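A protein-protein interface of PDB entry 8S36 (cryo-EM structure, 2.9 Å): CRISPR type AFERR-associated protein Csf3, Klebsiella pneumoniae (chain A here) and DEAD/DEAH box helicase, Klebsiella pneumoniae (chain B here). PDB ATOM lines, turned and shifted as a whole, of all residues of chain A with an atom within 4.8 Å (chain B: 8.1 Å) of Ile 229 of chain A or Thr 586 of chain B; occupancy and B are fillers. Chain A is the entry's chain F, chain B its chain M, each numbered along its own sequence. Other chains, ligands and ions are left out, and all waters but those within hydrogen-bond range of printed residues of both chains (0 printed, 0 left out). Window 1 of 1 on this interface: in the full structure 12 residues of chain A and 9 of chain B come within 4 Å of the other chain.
OH of Tyr 132 of chain A lies close to O of Leu 588 of chain B (3.5 Å). The side-chain hydroxyl (OH) of Tyr 132 of chain A sits at hydrogen-bond distance from the backbone NH (N) of Ser 589 of chain B (2.5 Å). The side-chain sulfur (SG) of Cys 624 of chain B lies within hydrogen-bond range of the side-chain amide oxygen (OE1) of Gln 227 of chain A. The backbone NH of Leu 228 of chain A lies close to the side-chain sulfur of Cys 624 of chain B (3.8 Å).
Of the printed residues of chain B, Tyr 132 of chain A touches Leu 588 and Ser 589. Printed residues of chain B within 4 Å of Leu 228 of chain A: Asp 621 and Cys 624. Printed residues of chain B within 4 Å of Ile 229 of chain A: Thr 586 (3.2 Å) and Leu 588 (3.999 Å). Printed residues of chain A within 4 Å of Thr 586 of chain B: Ile 229 and Ser 230. Of the printed residues of chain A, Leu 588 of chain B touches Tyr 132 and Ile 229. Ser 590 of chain B touches none of the printed residues of chain A. Tyr 617 of chain B touches none of the printed residues of chain A. Printed residues of chain A within 4 Å of Cys 624 of chain B: Ile 72, Gln 227 and Leu 228. The nearest printed residue of chain B that does not touch Ile 229 of chain A is Asp 587 of chain B (5.4 Å).
Printed residues of chain A that touch a printed residue of chain B: Ile 72, Tyr 132, Gln 227, Leu 228, Ile 229, Ser 230 and Leu 233. Hydrophobic or aromatic side chains of chain A that line the printed part of chain B: Ile 72, Tyr 132, Leu 228, Ile 229 and Leu 233. Among the printed residues, no Asp or Glu carboxylate lies within 4 Å of a Lys or Arg side-chain nitrogen of the other chain.
Cys 624 of chain B touches Ile 72 of chain A (C to CD1, 3.7 Å). CD1 of Leu 228 of chain A touches OD2 of Asp 621 of chain B, at 3.5 Å. Thr 586 of chain B touches Ile 229 of chain A (O to CG2, 3.2 Å). Ile 229 of chain A touches Leu 588 of chain B. Ser 230 of chain A touches Thr 586 of chain B. Pro 585 of chain B touches Leu 233 of chain A (O to CD2, 2.8 Å).
N of Gly 71 of chain A sits at hydrogen-bond distance from O of Tyr 132 of chain A (2.8 Å). The backbone carbonyl oxygen (O) of Gln 227 of chain A sits at hydrogen-bond distance from the backbone NH (N) of Ile 72 of chain A. The backbone carbonyl oxygen (O) of Ile 72 of chain A sits at hydrogen-bond distance from the backbone NH (N) of Ile 229 of chain A. OD1 of Asp 587 of chain B lies close to N of Ser 589 of chain B (3.4 Å).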
ATOM      1  N   ILE A  10      -2.147 -14.734  31.287  1.00  0.00           N
ATOM      2  CA  ILE A  10      -2.431 -13.893  30.133  1.00  0.00           C
ATOM      3  C   ILE A  10      -2.424 -12.449  30.602  1.00  0.00           C
ATOM      4  O   ILE A  10      -3.116 -12.102  31.566  1.00  0.00           O
ATOM      5  CB  ILE A  10      -3.778 -14.257  29.485  1.00  0.00           C
ATOM      6  CG1 ILE A  10      -3.805 -15.748  29.131  1.00  0.00           C
ATOM      7  CG2 ILE A  10      -4.016 -13.403  28.244  1.00  0.00           C
ATOM      8  CD1 ILE A  10      -5.155 -16.261  28.760  1.00  0.00           C
ATOM      9  N   GLY A  71      -1.437 -13.722  22.293  1.00  0.00           N
ATOM     10  CA  GLY A  71      -2.870 -13.883  22.226  1.00  0.00           C
ATOM     11  C   GLY A  71      -3.467 -12.761  21.409  1.00  0.00           C
ATOM     12  O   GLY A  71      -3.445 -11.589  21.821  1.00  0.00           O
ATOM     13  N   ILE A  72      -3.973 -13.121  20.232  1.00  0.00           N
ATOM     14  CA  ILE A  72      -4.523 -12.180  19.264  1.00  0.00           C
ATOM     15  C   ILE A  72      -6.037 -12.327  19.259  1.00  0.00           C
ATOM     16  O   ILE A  72      -6.560 -13.446  19.215  1.00  0.00           O
ATOM     17  CB  ILE A  72      -3.939 -12.411  17.858  1.00  0.00           C
ATOM     18  CG1 ILE A  72      -4.002 -13.894  17.472  1.00  0.00           C
ATOM     19  CG2 ILE A  72      -2.503 -11.922  17.799  1.00  0.00           C
ATOM     20  CD1 ILE A  72      -3.764 -14.152  16.004  1.00  0.00           C
ATOM     21  N   THR A  73      -6.730 -11.207  19.319  1.00  0.00           N
ATOM     22  CA  THR A  73      -8.180 -11.147  19.304  1.00  0.00           C
ATOM     23  C   THR A  73      -8.689 -10.857  17.900  1.00  0.00           C
ATOM     24  O   THR A  73      -7.924 -10.470  17.013  1.00  0.00           O
ATOM     25  CB  THR A  73      -8.657 -10.076  20.282  1.00  0.00           C
ATOM     26  OG1 THR A  73      -8.350  -8.776  19.764  1.00  0.00           O
ATOM     27  CG2 THR A  73      -7.972 -10.260  21.613  1.00  0.00           C
ATOM     28  N   TYR A 132      -2.410  -9.355  23.545  1.00  0.00           N
ATOM     29  CA  TYR A 132      -2.184 -10.120  24.765  1.00  0.00           C
ATOM     30  C   TYR A 132      -0.926 -10.962  24.635  1.00  0.00           C
ATOM     31  O   TYR A 132      -0.551 -11.379  23.541  1.00  0.00           O
ATOM     32  CB  TYR A 132      -3.387 -11.005  25.094  1.00  0.00           C
ATOM     33  CG  TYR A 132      -4.628 -10.187  25.304  1.00  0.00           C
ATOM     34  CD1 TYR A 132      -4.881  -9.577  26.522  1.00  0.00           C
ATOM     35  CD2 TYR A 132      -5.527  -9.987  24.272  1.00  0.00           C
ATOM     36  CE1 TYR A 132      -6.009  -8.812  26.711  1.00  0.00           C
ATOM     37  CE2 TYR A 132      -6.652  -9.225  24.452  1.00  0.00           C
ATOM     38  CZ  TYR A 132      -6.887  -8.637  25.666  1.00  0.00           C
ATOM     39  OH  TYR A 132      -8.018  -7.881  25.827  1.00  0.00           O
ATOM     40  N   GLN A 227      -2.076 -17.282  19.016  1.00  0.00           N
ATOM     41  CA  GLN A 227      -3.279 -18.064  19.255  1.00  0.00           C
ATOM     42  C   GLN A 227      -4.443 -17.112  19.479  1.00  0.00           C
ATOM     43  O   GLN A 227      -4.269 -16.009  20.003  1.00  0.00           O
ATOM     44  CB  GLN A 227      -3.111 -18.990  20.468  1.00  0.00           C
ATOM     45  CG  GLN A 227      -4.171 -20.073  20.590  1.00  0.00           C
ATOM     46  CD  GLN A 227      -3.910 -21.249  19.672  1.00  0.00           C
ATOM     47  OE1 GLN A 227      -4.543 -21.386  18.627  1.00  0.00           O
ATOM     48  NE2 GLN A 227      -2.973 -22.105  20.061  1.00  0.00           N
ATOM     49  N   LEU A 228      -5.635 -17.549  19.081  1.00  0.00           N
ATOM     50  CA  LEU A 228      -6.835 -16.781  19.383  1.00  0.00           C
ATOM     51  C   LEU A 228      -7.034 -16.705  20.890  1.00  0.00           C
ATOM     52  O   LEU A 228      -6.803 -17.678  21.613  1.00  0.00           O
ATOM     53  CB  LEU A 228      -8.059 -17.412  18.717  1.00  0.00           C
ATOM     54  CG  LEU A 228      -8.517 -16.808  17.385  1.00  0.00           C
ATOM     55  CD1 LEU A 228      -8.921 -15.346  17.545  1.00  0.00           C
ATOM     56  CD2 LEU A 228      -7.440 -16.954  16.317  1.00  0.00           C
ATOM     57  N   ILE A 229      -7.470 -15.536  21.367  1.00  0.00           N
ATOM     58  CA  ILE A 229      -7.681 -15.370  22.800  1.00  0.00           C
ATOM     59  C   ILE A 229      -8.771 -16.310  23.293  1.00  0.00           C
ATOM     60  O   ILE A 229      -8.725 -16.784  24.436  1.00  0.00           O
ATOM     61  CB  ILE A 229      -8.008 -13.894  23.114  1.00  0.00           C
ATOM     62  CG1 ILE A 229      -7.736 -13.581  24.585  1.00  0.00           C
ATOM     63  CG2 ILE A 229      -9.453 -13.572  22.762  1.00  0.00           C
ATOM     64  CD1 ILE A 229      -6.267 -13.437  24.919  1.00  0.00           C
ATOM     65  N   SER A 230      -9.754 -16.615  22.441  1.00  0.00           N
ATOM     66  CA  SER A 230     -10.777 -17.586  22.813  1.00  0.00           C
ATOM     67  C   SER A 230     -10.167 -18.962  23.038  1.00  0.00           C
ATOM     68  O   SER A 230     -10.506 -19.652  24.008  1.00  0.00           O
ATOM     69  CB  SER A 230     -11.855 -17.646  21.734  1.00  0.00           C
ATOM     70  OG  SER A 230     -11.278 -17.668  20.440  1.00  0.00           O
ATOM     71  N   SER A 231      -9.253 -19.374  22.158  1.00  0.00           N
ATOM     72  CA  SER A 231      -8.628 -20.681  22.308  1.00  0.00           C
ATOM     73  C   SER A 231      -7.714 -20.723  23.523  1.00  0.00           C
ATOM     74  O   SER A 231      -7.559 -21.779  24.144  1.00  0.00           O
ATOM     75  CB  SER A 231      -7.844 -21.035  21.044  1.00  0.00           C
ATOM     76  OG  SER A 231      -8.719 -21.396  19.989  1.00  0.00           O
ATOM     77  N   LEU A 232      -7.106 -19.590  23.877  1.00  0.00           N
ATOM     78  CA  LEU A 232      -6.260 -19.555  25.061  1.00  0.00           C
ATOM     79  C   LEU A 232      -7.097 -19.607  26.332  1.00  0.00           C
ATOM     80  O   LEU A 232      -6.699 -20.240  27.317  1.00  0.00           O
ATOM     81  CB  LEU A 232      -5.390 -18.300  25.043  1.00  0.00           C
ATOM     82  CG  LEU A 232      -4.402 -18.212  23.879  1.00  0.00           C
ATOM     83  CD1 LEU A 232      -3.813 -16.813  23.792  1.00  0.00           C
ATOM     84  CD2 LEU A 232      -3.311 -19.266  24.022  1.00  0.00           C
ATOM     85  N   LEU A 233      -8.258 -18.952  26.331  1.00  0.00           N
ATOM     86  CA  LEU A 233      -9.137 -18.990  27.491  1.00  0.00           C
ATOM     87  C   LEU A 233      -9.985 -20.252  27.553  1.00  0.00           C
ATOM     88  O   LEU A 233     -10.645 -20.482  28.572  1.00  0.00           O
ATOM     89  CB  LEU A 233     -10.054 -17.766  27.501  1.00  0.00           C
ATOM     90  CG  LEU A 233      -9.487 -16.541  28.216  1.00  0.00           C
ATOM     91  CD1 LEU A 233      -8.158 -16.124  27.620  1.00  0.00           C
ATOM     92  CD2 LEU A 233     -10.468 -15.403  28.152  1.00  0.00           C
ATOM     93  N   ILE B 402     -24.197 -15.166  30.360  1.00  0.00           N
ATOM     94  CA  ILE B 402     -24.042 -13.723  30.206  1.00  0.00           C
ATOM     95  C   ILE B 402     -24.415 -13.324  28.788  1.00  0.00           C
ATOM     96  O   ILE B 402     -24.132 -14.050  27.831  1.00  0.00           O
ATOM     97  CB  ILE B 402     -22.606 -13.253  30.517  1.00  0.00           C
ATOM     98  CG1 ILE B 402     -21.585 -14.172  29.843  1.00  0.00           C
ATOM     99  CG2 ILE B 402     -22.380 -13.189  32.013  1.00  0.00           C
ATOM    100  CD1 ILE B 402     -20.287 -13.487  29.495  1.00  0.00           C
ATOM    101  N   PRO B 583     -18.520  -7.900  30.647  1.00  0.00           N
ATOM    102  CA  PRO B 583     -17.402  -8.363  29.817  1.00  0.00           C
ATOM    103  C   PRO B 583     -17.523  -9.847  29.503  1.00  0.00           C
ATOM    104  O   PRO B 583     -17.701 -10.674  30.399  1.00  0.00           O
ATOM    105  CB  PRO B 583     -16.174  -8.069  30.683  1.00  0.00           C
ATOM    106  CG  PRO B 583     -16.689  -8.122  32.072  1.00  0.00           C
ATOM    107  CD  PRO B 583     -18.064  -7.529  31.999  1.00  0.00           C
ATOM    108  N   GLU B 584     -17.425 -10.175  28.220  1.00  0.00           N
ATOM    109  CA  GLU B 584     -17.292 -11.562  27.818  1.00  0.00           C
ATOM    110  C   GLU B 584     -15.960 -12.117  28.322  1.00  0.00           C
ATOM    111  O   GLU B 584     -15.005 -11.363  28.525  1.00  0.00           O
ATOM    112  CB  GLU B 584     -17.372 -11.694  26.300  1.00  0.00           C
ATOM    113  CG  GLU B 584     -18.653 -11.140  25.698  1.00  0.00           C
ATOM    114  CD  GLU B 584     -18.729 -11.345  24.198  1.00  0.00           C
ATOM    115  OE1 GLU B 584     -17.786 -11.935  23.628  1.00  0.00           O
ATOM    116  OE2 GLU B 584     -19.732 -10.919  23.588  1.00  0.00           O
ATOM    117  N   PRO B 585     -15.870 -13.432  28.547  1.00  0.00           N
ATOM    118  CA  PRO B 585     -14.556 -13.999  28.891  1.00  0.00           C
ATOM    119  C   PRO B 585     -13.505 -13.704  27.839  1.00  0.00           C
ATOM    120  O   PRO B 585     -12.372 -13.344  28.181  1.00  0.00           O
ATOM    121  CB  PRO B 585     -14.842 -15.503  29.008  1.00  0.00           C
ATOM    122  CG  PRO B 585     -16.289 -15.600  29.284  1.00  0.00           C
ATOM    123  CD  PRO B 585     -16.932 -14.450  28.579  1.00  0.00           C
ATOM    124  N   THR B 586     -13.871 -13.789  26.560  1.00  0.00           N
ATOM    125  CA  THR B 586     -12.897 -13.651  25.485  1.00  0.00           C
ATOM    126  C   THR B 586     -12.495 -12.200  25.259  1.00  0.00           C
ATOM    127  O   THR B 586     -11.385 -11.940  24.782  1.00  0.00           O
ATOM    128  CB  THR B 586     -13.456 -14.238  24.188  1.00  0.00           C
ATOM    129  OG1 THR B 586     -14.572 -13.456  23.747  1.00  0.00           O
ATOM    130  CG2 THR B 586     -13.901 -15.678  24.399  1.00  0.00           C
ATOM    131  N   ASP B 587     -13.367 -11.249  25.591  1.00  0.00           N
ATOM    132  CA  ASP B 587     -13.078  -9.830  25.393  1.00  0.00           C
ATOM    133  C   ASP B 587     -12.422  -9.310  26.664  1.00  0.00           C
ATOM    134  O   ASP B 587     -13.071  -8.758  27.553  1.00  0.00           O
ATOM    135  CB  ASP B 587     -14.349  -9.061  25.057  1.00  0.00           C
ATOM    136  CG  ASP B 587     -14.065  -7.667  24.527  1.00  0.00           C
ATOM    137  OD1 ASP B 587     -13.192  -6.976  25.093  1.00  0.00           O
ATOM    138  OD2 ASP B 587     -14.717  -7.262  23.542  1.00  0.00           O
ATOM    139  N   LEU B 588     -11.104  -9.491  26.742  1.00  0.00           N
ATOM    140  CA  LEU B 588     -10.318  -9.046  27.885  1.00  0.00           C
ATOM    141  C   LEU B 588      -9.976  -7.562  27.828  1.00  0.00           C
ATOM    142  O   LEU B 588      -9.541  -7.003  28.840  1.00  0.00           O
ATOM    143  CB  LEU B 588      -9.036  -9.876  27.985  1.00  0.00           C
ATOM    144  CG  LEU B 588      -9.192 -11.239  28.662  1.00  0.00           C
ATOM    145  CD1 LEU B 588      -8.025 -12.147  28.307  1.00  0.00           C
ATOM    146  CD2 LEU B 588      -9.307 -11.084  30.171  1.00  0.00           C
ATOM    147  N   SER B 589     -10.142  -6.918  26.673  1.00  0.00           N
ATOM    148  CA  SER B 589      -9.887  -5.492  26.520  1.00  0.00           C
ATOM    149  C   SER B 589     -11.167  -4.671  26.598  1.00  0.00           C
ATOM    150  O   SER B 589     -11.157  -3.485  26.254  1.00  0.00           O
ATOM    151  CB  SER B 589      -9.175  -5.223  25.192  1.00  0.00           C
ATOM    152  OG  SER B 589      -9.793  -5.930  24.131  1.00  0.00           O
ATOM    153  N   SER B 590     -12.263  -5.276  27.047  1.00  0.00           N
ATOM    154  CA  SER B 590     -13.511  -4.550  27.223  1.00  0.00           C
ATOM    155  C   SER B 590     -13.348  -3.457  28.271  1.00  0.00           C
ATOM    156  O   SER B 590     -12.578  -3.590  29.227  1.00  0.00           O
ATOM    157  CB  SER B 590     -14.627  -5.508  27.635  1.00  0.00           C
ATOM    158  OG  SER B 590     -14.328  -6.123  28.874  1.00  0.00           O
ATOM    159  N   ARG B 593     -13.770  -4.266  32.190  1.00  0.00           N
ATOM    160  CA  ARG B 593     -13.088  -5.523  32.473  1.00  0.00           C
ATOM    161  C   ARG B 593     -13.142  -5.873  33.951  1.00  0.00           C
ATOM    162  O   ARG B 593     -13.043  -7.050  34.306  1.00  0.00           O
ATOM    163  CB  ARG B 593     -11.632  -5.443  32.010  1.00  0.00           C
ATOM    164  CG  ARG B 593     -10.856  -6.754  32.127  1.00  0.00           C
ATOM    165  CD  ARG B 593     -11.331  -7.788  31.124  1.00  0.00           C
ATOM    166  NE  ARG B 593     -11.995  -8.920  31.760  1.00  0.00           N
ATOM    167  CZ  ARG B 593     -12.832  -9.746  31.144  1.00  0.00           C
ATOM    168  NH1 ARG B 593     -13.141  -9.597  29.865  1.00  0.00           N
ATOM    169  NH2 ARG B 593     -13.369 -10.753  31.827  1.00  0.00           N
ATOM    170  N   TYR B 607     -17.149 -18.871  34.901  1.00  0.00           N
ATOM    171  CA  TYR B 607     -17.134 -17.652  34.103  1.00  0.00           C
ATOM    172  C   TYR B 607     -16.437 -17.900  32.773  1.00  0.00           C
ATOM    173  O   TYR B 607     -16.887 -17.420  31.727  1.00  0.00           O
ATOM    174  CB  TYR B 607     -16.458 -16.509  34.859  1.00  0.00           C
ATOM    175  CG  TYR B 607     -16.262 -15.276  34.007  1.00  0.00           C
ATOM    176  CD1 TYR B 607     -17.321 -14.719  33.305  1.00  0.00           C
ATOM    177  CD2 TYR B 607     -15.015 -14.678  33.890  1.00  0.00           C
ATOM    178  CE1 TYR B 607     -17.148 -13.597  32.520  1.00  0.00           C
ATOM    179  CE2 TYR B 607     -14.831 -13.555  33.106  1.00  0.00           C
ATOM    180  CZ  TYR B 607     -15.902 -13.020  32.424  1.00  0.00           C
ATOM    181  OH  TYR B 607     -15.727 -11.901  31.641  1.00  0.00           O
ATOM    182  N   ARG B 608     -15.337 -18.657  32.793  1.00  0.00           N
ATOM    183  CA  ARG B 608     -14.596 -18.919  31.567  1.00  0.00           C
ATOM    184  C   ARG B 608     -15.287 -19.961  30.699  1.00  0.00           C
ATOM    185  O   ARG B 608     -15.117 -19.951  29.474  1.00  0.00           O
ATOM    186  CB  ARG B 608     -13.176 -19.378  31.903  1.00  0.00           C
ATOM    187  CG  ARG B 608     -12.192 -18.240  32.106  1.00  0.00           C
ATOM    188  CD  ARG B 608     -10.785 -18.766  32.325  1.00  0.00           C
ATOM    189  NE  ARG B 608     -10.698 -19.585  33.529  1.00  0.00           N
ATOM    190  CZ  ARG B 608     -10.646 -19.105  34.765  1.00  0.00           C
ATOM    191  NH1 ARG B 608     -10.658 -17.803  35.005  1.00  0.00           N
ATOM    192  NH2 ARG B 608     -10.582 -19.953  35.788  1.00  0.00           N
ATOM    193  N   CYS B 610     -18.867 -20.615  29.974  1.00  0.00           N
ATOM    194  CA  CYS B 610     -20.200 -20.065  30.158  1.00  0.00           C
ATOM    195  C   CYS B 610     -20.965 -20.110  28.844  1.00  0.00           C
ATOM    196  O   CYS B 610     -20.388 -20.261  27.764  1.00  0.00           O
ATOM    197  CB  CYS B 610     -20.141 -18.622  30.670  1.00  0.00           C
ATOM    198  SG  CYS B 610     -19.391 -17.456  29.511  1.00  0.00           S
ATOM    199  N   ILE B 612     -23.237 -17.969  26.285  1.00  0.00           N
ATOM    200  CA  ILE B 612     -23.457 -16.591  25.865  1.00  0.00           C
ATOM    201  C   ILE B 612     -24.682 -16.567  24.966  1.00  0.00           C
ATOM    202  O   ILE B 612     -24.750 -17.304  23.974  1.00  0.00           O
ATOM    203  CB  ILE B 612     -22.229 -16.001  25.148  1.00  0.00           C
ATOM    204  CG1 ILE B 612     -20.968 -16.164  26.005  1.00  0.00           C
ATOM    205  CG2 ILE B 612     -22.460 -14.521  24.852  1.00  0.00           C
ATOM    206  CD1 ILE B 612     -19.678 -15.852  25.271  1.00  0.00           C
ATOM    207  N   PRO B 615     -23.570 -13.759  21.707  1.00  0.00           N
ATOM    208  CA  PRO B 615     -22.125 -13.530  21.588  1.00  0.00           C
ATOM    209  C   PRO B 615     -21.792 -12.774  20.316  1.00  0.00           C
ATOM    210  O   PRO B 615     -22.690 -12.454  19.531  1.00  0.00           O
ATOM    211  CB  PRO B 615     -21.544 -14.949  21.571  1.00  0.00           C
ATOM    212  CG  PRO B 615     -22.641 -15.788  21.017  1.00  0.00           C
ATOM    213  CD  PRO B 615     -23.920 -15.177  21.515  1.00  0.00           C
ATOM    214  N   ALA B 616     -20.513 -12.484  20.099  1.00  0.00           N
ATOM    215  CA  ALA B 616     -20.072 -11.819  18.886  1.00  0.00           C
ATOM    216  C   ALA B 616     -18.835 -12.518  18.350  1.00  0.00           C
ATOM    217  O   ALA B 616     -18.105 -13.184  19.089  1.00  0.00           O
ATOM    218  CB  ALA B 616     -19.766 -10.337  19.140  1.00  0.00           C
ATOM    219  N   TYR B 617     -18.596 -12.316  17.058  1.00  0.00           N
ATOM    220  CA  TYR B 617     -17.455 -12.881  16.337  1.00  0.00           C
ATOM    221  C   TYR B 617     -17.206 -14.327  16.764  1.00  0.00           C
ATOM    222  O   TYR B 617     -16.124 -14.704  17.214  1.00  0.00           O
ATOM    223  CB  TYR B 617     -16.197 -12.026  16.531  1.00  0.00           C
ATOM    224  CG  TYR B 617     -16.374 -10.511  16.445  1.00  0.00           C
ATOM    225  CD1 TYR B 617     -17.483  -9.933  15.829  1.00  0.00           C
ATOM    226  CD2 TYR B 617     -15.428  -9.658  17.001  1.00  0.00           C
ATOM    227  CE1 TYR B 617     -17.635  -8.563  15.762  1.00  0.00           C
ATOM    228  CE2 TYR B 617     -15.574  -8.285  16.938  1.00  0.00           C
ATOM    229  CZ  TYR B 617     -16.680  -7.743  16.318  1.00  0.00           C
ATOM    230  OH  TYR B 617     -16.830  -6.377  16.253  1.00  0.00           O
ATOM    231  N   ASP B 621     -11.082 -17.492  13.008  1.00  0.00           N
ATOM    232  CA  ASP B 621     -10.144 -16.641  12.291  1.00  0.00           C
ATOM    233  C   ASP B 621      -8.960 -17.481  11.836  1.00  0.00           C
ATOM    234  O   ASP B 621      -8.383 -18.232  12.628  1.00  0.00           O
ATOM    235  CB  ASP B 621      -9.675 -15.488  13.176  1.00  0.00           C
ATOM    236  CG  ASP B 621     -10.822 -14.642  13.687  1.00  0.00           C
ATOM    237  OD1 ASP B 621     -11.852 -14.554  12.987  1.00  0.00           O
ATOM    238  OD2 ASP B 621     -10.696 -14.066  14.787  1.00  0.00           O
ATOM    239  N   CYS B 624      -4.394 -17.387  12.985  1.00  0.00           N
ATOM    240  CA  CYS B 624      -4.321 -17.831  14.371  1.00  0.00           C
ATOM    241  C   CYS B 624      -2.937 -17.575  14.952  1.00  0.00           C
ATOM    242  O   CYS B 624      -1.936 -17.626  14.238  1.00  0.00           O
ATOM    243  CB  CYS B 624      -4.664 -19.318  14.473  1.00  0.00           C
ATOM    244  SG  CYS B 624      -5.278 -19.829  16.093  1.00  0.00           S
